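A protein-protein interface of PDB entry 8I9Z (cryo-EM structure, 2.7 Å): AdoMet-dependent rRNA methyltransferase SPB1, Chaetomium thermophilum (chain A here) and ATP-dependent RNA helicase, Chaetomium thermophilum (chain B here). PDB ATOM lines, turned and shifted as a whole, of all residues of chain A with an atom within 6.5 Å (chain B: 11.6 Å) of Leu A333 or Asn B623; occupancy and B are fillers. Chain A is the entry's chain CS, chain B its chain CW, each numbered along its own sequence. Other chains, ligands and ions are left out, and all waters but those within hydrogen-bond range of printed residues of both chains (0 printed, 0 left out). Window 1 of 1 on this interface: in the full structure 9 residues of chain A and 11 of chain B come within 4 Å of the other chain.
The guanidinium group of Arg B620 sits at hydrogen-bond distance from the backbone carbonyl oxygen of Ile A330 (3.1 Å). The backbone carbonyl oxygen of Phe A331 lies close to the side-chain amide oxygen of Asn B623, 2.9 Å away.
Of the printed residues of chain B, Leu A333 touches Asn B623 (3.8 Å). Asn B623 touches two residues of chain A. No residue of chain B comes within 4 Å of Asn A263. Of chain B, only Ile B616 (3.9 Å), Val B619 (3.8 Å), Arg B620 (3.3 Å) and Asn B623 (2.9 Å) come within 4 Å of Phe A331. No residue of chain B comes within 4 Å of Gly A332. No residue of chain B comes within 4 Å of Pro A334. Of the printed residues of chain A, Val B619 touches Phe A331 (3.8 Å). Of the printed residues of chain B, Ile A330 touches Ile B616 and Arg B620. Printed residues of chain A within 4 Å of Arg B620: Ile A330 (3.1 Å) and Phe A331 (3.3 Å). Of the printed residues of chain A, Ile B616 touches Ile A330 and Phe A331. The nearest residue of chain B that does not touch Leu A333 is Gln B624 (6.8 Å).
The backbone NH of Leu A333 sits at hydrogen-bond distance from the backbone carbonyl oxygen of Arg A328 (3.2 Å). The side-chain amide oxygen of Asn B623 lies close to the backbone carbonyl oxygen of Val B619, at 2.8 Å.
Of the 10 printed residues of chain B, 4 touch a printed residue of chain A. Printed residues of chain B that touch a printed residue of chain A: Ile B616, Val B619, Arg B620 and Asn B623. Hydrophobic or aromatic side chains of chain B within 4 Å of the printed part of chain A: Ile B616 and Val B619. Hydrophobic or aromatic side chains of chain A within 4 Å of the printed part of chain B: Ile A330, Phe A331 and Leu A333. Among the printed residues, no Asp or Glu carboxylate lies within 4 Å of a Lys or Arg side-chain nitrogen of the other chain.
Among the printed residues, merely in contact across the chains: Ile A330 with Ile B616, Phe A331 with Ile B616, Phe A331 with Val B619, Phe A331 with Arg B620 and Leu A333 with Asn B623.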
ATOM      1  N   ILE A 262     -29.204   9.102 -31.827  1.00  0.00           N
ATOM      2  CA  ILE A 262     -29.810   7.797 -31.581  1.00  0.00           C
ATOM      3  C   ILE A 262     -29.974   7.550 -30.087  1.00  0.00           C
ATOM      4  O   ILE A 262     -31.015   7.058 -29.636  1.00  0.00           O
ATOM      5  CB  ILE A 262     -28.967   6.703 -32.254  1.00  0.00           C
ATOM      6  CG1 ILE A 262     -28.858   6.989 -33.747  1.00  0.00           C
ATOM      7  CG2 ILE A 262     -29.570   5.331 -32.014  1.00  0.00           C
ATOM      8  CD1 ILE A 262     -28.120   5.944 -34.512  1.00  0.00           C
ATOM      9  N   ASN A 263     -28.962   7.901 -29.295  1.00  0.00           N
ATOM     10  CA  ASN A 263     -28.952   7.573 -27.876  1.00  0.00           C
ATOM     11  C   ASN A 263     -29.834   8.480 -27.033  1.00  0.00           C
ATOM     12  O   ASN A 263     -30.046   8.180 -25.855  1.00  0.00           O
ATOM     13  CB  ASN A 263     -27.523   7.620 -27.334  1.00  0.00           C
ATOM     14  CG  ASN A 263     -26.757   6.335 -27.587  1.00  0.00           C
ATOM     15  OD1 ASN A 263     -26.862   5.740 -28.658  1.00  0.00           O
ATOM     16  ND2 ASN A 263     -25.982   5.901 -26.603  1.00  0.00           N
ATOM     17  N   VAL A 327     -32.236   1.492 -36.019  1.00  0.00           N
ATOM     18  CA  VAL A 327     -30.913   1.283 -35.440  1.00  0.00           C
ATOM     19  C   VAL A 327     -31.029   0.896 -33.971  1.00  0.00           C
ATOM     20  O   VAL A 327     -30.279   0.044 -33.479  1.00  0.00           O
ATOM     21  CB  VAL A 327     -30.037   2.534 -35.640  1.00  0.00           C
ATOM     22  CG1 VAL A 327     -28.659   2.332 -35.032  1.00  0.00           C
ATOM     23  CG2 VAL A 327     -29.905   2.851 -37.113  1.00  0.00           C
ATOM     24  N   ARG A 328     -31.973   1.506 -33.249  1.00  0.00           N
ATOM     25  CA  ARG A 328     -32.208   1.125 -31.860  1.00  0.00           C
ATOM     26  C   ARG A 328     -32.723  -0.304 -31.756  1.00  0.00           C
ATOM     27  O   ARG A 328     -32.430  -1.009 -30.783  1.00  0.00           O
ATOM     28  CB  ARG A 328     -33.186   2.096 -31.206  1.00  0.00           C
ATOM     29  CG  ARG A 328     -32.589   3.450 -30.904  1.00  0.00           C
ATOM     30  CD  ARG A 328     -33.637   4.404 -30.385  1.00  0.00           C
ATOM     31  NE  ARG A 328     -34.045   4.083 -29.026  1.00  0.00           N
ATOM     32  CZ  ARG A 328     -33.545   4.662 -27.944  1.00  0.00           C
ATOM     33  NH1 ARG A 328     -32.605   5.589 -28.030  1.00  0.00           N
ATOM     34  NH2 ARG A 328     -33.997   4.301 -26.747  1.00  0.00           N
ATOM     35  N   GLU A 329     -33.504  -0.747 -32.743  1.00  0.00           N
ATOM     36  CA  GLU A 329     -33.859  -2.159 -32.823  1.00  0.00           C
ATOM     37  C   GLU A 329     -32.627  -3.013 -33.089  1.00  0.00           C
ATOM     38  O   GLU A 329     -32.508  -4.125 -32.562  1.00  0.00           O
ATOM     39  CB  GLU A 329     -34.911  -2.375 -33.910  1.00  0.00           C
ATOM     40  CG  GLU A 329     -36.327  -2.017 -33.491  1.00  0.00           C
ATOM     41  CD  GLU A 329     -37.301  -2.045 -34.654  1.00  0.00           C
ATOM     42  OE1 GLU A 329     -36.858  -2.298 -35.795  1.00  0.00           O
ATOM     43  OE2 GLU A 329     -38.507  -1.812 -34.427  1.00  0.00           O
ATOM     44  N   ILE A 330     -31.705  -2.512 -33.912  1.00  0.00           N
ATOM     45  CA  ILE A 330     -30.454  -3.226 -34.157  1.00  0.00           C
ATOM     46  C   ILE A 330     -29.580  -3.212 -32.910  1.00  0.00           C
ATOM     47  O   ILE A 330     -29.059  -4.249 -32.484  1.00  0.00           O
ATOM     48  CB  ILE A 330     -29.719  -2.624 -35.370  1.00  0.00           C
ATOM     49  CG1 ILE A 330     -30.363  -3.074 -36.680  1.00  0.00           C
ATOM     50  CG2 ILE A 330     -28.252  -2.993 -35.362  1.00  0.00           C
ATOM     51  CD1 ILE A 330     -29.560  -2.690 -37.909  1.00  0.00           C
ATOM     52  N   PHE A 331     -29.420  -2.042 -32.293  1.00  0.00           N
ATOM     53  CA  PHE A 331     -28.466  -1.897 -31.200  1.00  0.00           C
ATOM     54  C   PHE A 331     -28.989  -2.419 -29.869  1.00  0.00           C
ATOM     55  O   PHE A 331     -28.184  -2.782 -29.005  1.00  0.00           O
ATOM     56  CB  PHE A 331     -28.052  -0.434 -31.051  1.00  0.00           C
ATOM     57  CG  PHE A 331     -26.975  -0.001 -32.008  1.00  0.00           C
ATOM     58  CD1 PHE A 331     -26.482  -0.870 -32.970  1.00  0.00           C
ATOM     59  CD2 PHE A 331     -26.457   1.279 -31.942  1.00  0.00           C
ATOM     60  CE1 PHE A 331     -25.494  -0.466 -33.845  1.00  0.00           C
ATOM     61  CE2 PHE A 331     -25.469   1.687 -32.813  1.00  0.00           C
ATOM     62  CZ  PHE A 331     -24.987   0.813 -33.766  1.00  0.00           C
ATOM     63  N   GLY A 332     -30.301  -2.454 -29.668  1.00  0.00           N
ATOM     64  CA  GLY A 332     -30.853  -3.046 -28.468  1.00  0.00           C
ATOM     65  C   GLY A 332     -31.315  -2.085 -27.397  1.00  0.00           C
ATOM     66  O   GLY A 332     -31.482  -2.506 -26.246  1.00  0.00           O
ATOM     67  N   LEU A 333     -31.517  -0.813 -27.727  1.00  0.00           N
ATOM     68  CA  LEU A 333     -32.106   0.118 -26.779  1.00  0.00           C
ATOM     69  C   LEU A 333     -33.568  -0.252 -26.525  1.00  0.00           C
ATOM     70  O   LEU A 333     -34.221  -0.839 -27.392  1.00  0.00           O
ATOM     71  CB  LEU A 333     -32.003   1.559 -27.285  1.00  0.00           C
ATOM     72  CG  LEU A 333     -30.662   2.252 -27.583  1.00  0.00           C
ATOM     73  CD1 LEU A 333     -29.750   2.210 -26.358  1.00  0.00           C
ATOM     74  CD2 LEU A 333     -29.933   1.786 -28.840  1.00  0.00           C
ATOM     75  N   PRO A 334     -34.092   0.047 -25.326  1.00  0.00           N
ATOM     76  CA  PRO A 334     -35.455  -0.410 -24.985  1.00  0.00           C
ATOM     77  C   PRO A 334     -36.558   0.135 -25.878  1.00  0.00           C
ATOM     78  O   PRO A 334     -37.525  -0.584 -26.161  1.00  0.00           O
ATOM     79  CB  PRO A 334     -35.624   0.066 -23.535  1.00  0.00           C
ATOM     80  CG  PRO A 334     -34.242   0.160 -23.008  1.00  0.00           C
ATOM     81  CD  PRO A 334     -33.410   0.632 -24.159  1.00  0.00           C
ATOM     82  N   SER A 335     -36.444   1.375 -26.340  1.00  0.00           N
ATOM     83  CA  SER A 335     -37.484   1.960 -27.178  1.00  0.00           C
ATOM     84  C   SER A 335     -36.924   3.062 -28.069  1.00  0.00           C
ATOM     85  O   SER A 335     -36.981   2.969 -29.295  1.00  0.00           O
ATOM     86  CB  SER A 335     -38.622   2.511 -26.315  1.00  0.00           C
ATOM     87  OG  SER A 335     -38.138   3.448 -25.368  1.00  0.00           O
ATOM     88  N   LEU B 615     -19.610  -6.193 -35.738  1.00  0.00           N
ATOM     89  CA  LEU B 615     -19.661  -4.828 -35.236  1.00  0.00           C
ATOM     90  C   LEU B 615     -20.898  -4.536 -34.400  1.00  0.00           C
ATOM     91  O   LEU B 615     -20.866  -3.611 -33.583  1.00  0.00           O
ATOM     92  CB  LEU B 615     -19.585  -3.825 -36.392  1.00  0.00           C
ATOM     93  CG  LEU B 615     -18.231  -3.149 -36.620  1.00  0.00           C
ATOM     94  CD1 LEU B 615     -17.958  -2.130 -35.524  1.00  0.00           C
ATOM     95  CD2 LEU B 615     -17.109  -4.168 -36.686  1.00  0.00           C
ATOM     96  N   ILE B 616     -21.988  -5.292 -34.558  1.00  0.00           N
ATOM     97  CA  ILE B 616     -23.134  -5.050 -33.687  1.00  0.00           C
ATOM     98  C   ILE B 616     -23.039  -5.878 -32.408  1.00  0.00           C
ATOM     99  O   ILE B 616     -23.440  -5.406 -31.343  1.00  0.00           O
ATOM    100  CB  ILE B 616     -24.509  -5.251 -34.371  1.00  0.00           C
ATOM    101  CG1 ILE B 616     -24.649  -4.657 -35.781  1.00  0.00           C
ATOM    102  CG2 ILE B 616     -25.622  -4.670 -33.527  1.00  0.00           C
ATOM    103  CD1 ILE B 616     -24.174  -5.457 -36.895  1.00  0.00           C
ATOM    104  N   ASN B 617     -22.478  -7.101 -32.460  1.00  0.00           N
ATOM    105  CA  ASN B 617     -22.696  -8.008 -31.325  1.00  0.00           C
ATOM    106  C   ASN B 617     -21.947  -7.566 -30.069  1.00  0.00           C
ATOM    107  O   ASN B 617     -22.132  -8.173 -29.008  1.00  0.00           O
ATOM    108  CB  ASN B 617     -22.311  -9.464 -31.627  1.00  0.00           C
ATOM    109  CG  ASN B 617     -21.130  -9.593 -32.543  1.00  0.00           C
ATOM    110  OD1 ASN B 617     -20.312  -8.688 -32.635  1.00  0.00           O
ATOM    111  ND2 ASN B 617     -21.022 -10.730 -33.226  1.00  0.00           N
ATOM    112  N   GLU B 618     -21.099  -6.532 -30.153  1.00  0.00           N
ATOM    113  CA  GLU B 618     -20.506  -6.014 -28.925  1.00  0.00           C
ATOM    114  C   GLU B 618     -21.252  -4.797 -28.397  1.00  0.00           C
ATOM    115  O   GLU B 618     -21.251  -4.565 -27.183  1.00  0.00           O
ATOM    116  CB  GLU B 618     -19.030  -5.616 -29.094  1.00  0.00           C
ATOM    117  CG  GLU B 618     -18.579  -4.684 -30.241  1.00  0.00           C
ATOM    118  CD  GLU B 618     -18.740  -5.198 -31.650  1.00  0.00           C
ATOM    119  OE1 GLU B 618     -18.027  -4.652 -32.511  1.00  0.00           O
ATOM    120  OE2 GLU B 618     -19.574  -6.086 -31.918  1.00  0.00           O
ATOM    121  N   VAL B 619     -21.871  -3.991 -29.269  1.00  0.00           N
ATOM    122  CA  VAL B 619     -22.531  -2.786 -28.770  1.00  0.00           C
ATOM    123  C   VAL B 619     -23.815  -3.151 -28.038  1.00  0.00           C
ATOM    124  O   VAL B 619     -24.303  -2.384 -27.201  1.00  0.00           O
ATOM    125  CB  VAL B 619     -22.781  -1.750 -29.890  1.00  0.00           C
ATOM    126  CG1 VAL B 619     -21.474  -1.097 -30.334  1.00  0.00           C
ATOM    127  CG2 VAL B 619     -23.551  -2.314 -31.067  1.00  0.00           C
ATOM    128  N   ARG B 620     -24.379  -4.330 -28.329  1.00  0.00           N
ATOM    129  CA  ARG B 620     -25.463  -4.843 -27.496  1.00  0.00           C
ATOM    130  C   ARG B 620     -24.990  -5.122 -26.080  1.00  0.00           C
ATOM    131  O   ARG B 620     -25.762  -4.960 -25.130  1.00  0.00           O
ATOM    132  CB  ARG B 620     -26.054  -6.123 -28.089  1.00  0.00           C
ATOM    133  CG  ARG B 620     -25.918  -6.239 -29.576  1.00  0.00           C
ATOM    134  CD  ARG B 620     -27.078  -5.569 -30.287  1.00  0.00           C
ATOM    135  NE  ARG B 620     -28.310  -6.353 -30.346  1.00  0.00           N
ATOM    136  CZ  ARG B 620     -28.451  -7.545 -30.916  1.00  0.00           C
ATOM    137  NH1 ARG B 620     -27.486  -8.097 -31.637  1.00  0.00           N
ATOM    138  NH2 ARG B 620     -29.615  -8.180 -30.806  1.00  0.00           N
ATOM    139  N   LYS B 621     -23.735  -5.554 -25.921  1.00  0.00           N
ATOM    140  CA  LYS B 621     -23.221  -5.872 -24.593  1.00  0.00           C
ATOM    141  C   LYS B 621     -23.146  -4.627 -23.719  1.00  0.00           C
ATOM    142  O   LYS B 621     -23.424  -4.689 -22.515  1.00  0.00           O
ATOM    143  CB  LYS B 621     -21.853  -6.544 -24.703  1.00  0.00           C
ATOM    144  CG  LYS B 621     -21.919  -8.026 -25.033  1.00  0.00           C
ATOM    145  CD  LYS B 621     -20.553  -8.678 -24.914  1.00  0.00           C
ATOM    146  CE  LYS B 621     -19.720  -8.453 -26.165  1.00  0.00           C
ATOM    147  NZ  LYS B 621     -20.257  -9.209 -27.330  1.00  0.00           N
ATOM    148  N   ARG B 622     -22.775  -3.487 -24.304  1.00  0.00           N
ATOM    149  CA  ARG B 622     -22.837  -2.231 -23.566  1.00  0.00           C
ATOM    150  C   ARG B 622     -24.276  -1.770 -23.370  1.00  0.00           C
ATOM    151  O   ARG B 622     -24.612  -1.209 -22.321  1.00  0.00           O
ATOM    152  CB  ARG B 622     -22.015  -1.158 -24.278  1.00  0.00           C
ATOM    153  CG  ARG B 622     -20.567  -1.094 -23.824  1.00  0.00           C
ATOM    154  CD  ARG B 622     -19.658  -1.981 -24.652  1.00  0.00           C
ATOM    155  NE  ARG B 622     -19.542  -1.535 -26.034  1.00  0.00           N
ATOM    156  CZ  ARG B 622     -18.940  -2.231 -26.988  1.00  0.00           C
ATOM    157  NH1 ARG B 622     -18.368  -3.396 -26.735  1.00  0.00           N
ATOM    158  NH2 ARG B 622     -18.903  -1.742 -28.224  1.00  0.00           N
ATOM    159  N   ASN B 623     -25.140  -1.989 -24.365  1.00  0.00           N
ATOM    160  CA  ASN B 623     -26.533  -1.573 -24.223  1.00  0.00           C
ATOM    161  C   ASN B 623     -27.291  -2.473 -23.253  1.00  0.00           C
ATOM    162  O   ASN B 623     -28.127  -1.992 -22.480  1.00  0.00           O
ATOM    163  CB  ASN B 623     -27.226  -1.543 -25.586  1.00  0.00           C
ATOM    164  CG  ASN B 623     -26.646  -0.494 -26.515  1.00  0.00           C
ATOM    165  OD1 ASN B 623     -26.538  -0.707 -27.723  1.00  0.00           O
ATOM    166  ND2 ASN B 623     -26.263   0.647 -25.954  1.00  0.00           N
ATOM    167  N   GLN B 624     -27.018  -3.774 -23.273  1.00  0.00           N
ATOM    168  CA  GLN B 624     -27.677  -4.695 -22.353  1.00  0.00           C
ATOM    169  C   GLN B 624     -26.835  -4.881 -21.097  1.00  0.00           C
ATOM    170  O   GLN B 624     -25.832  -4.194 -20.907  1.00  0.00           O
ATOM    171  CB  GLN B 624     -27.932  -6.049 -23.021  1.00  0.00           C
ATOM    172  CG  GLN B 624     -28.979  -6.014 -24.123  1.00  0.00           C
ATOM    173  CD  GLN B 624     -29.195  -7.372 -24.763  1.00  0.00           C
ATOM    174  OE1 GLN B 624     -28.493  -8.335 -24.455  1.00  0.00           O
ATOM    175  NE2 GLN B 624     -30.171  -7.454 -25.660  1.00  0.00           N
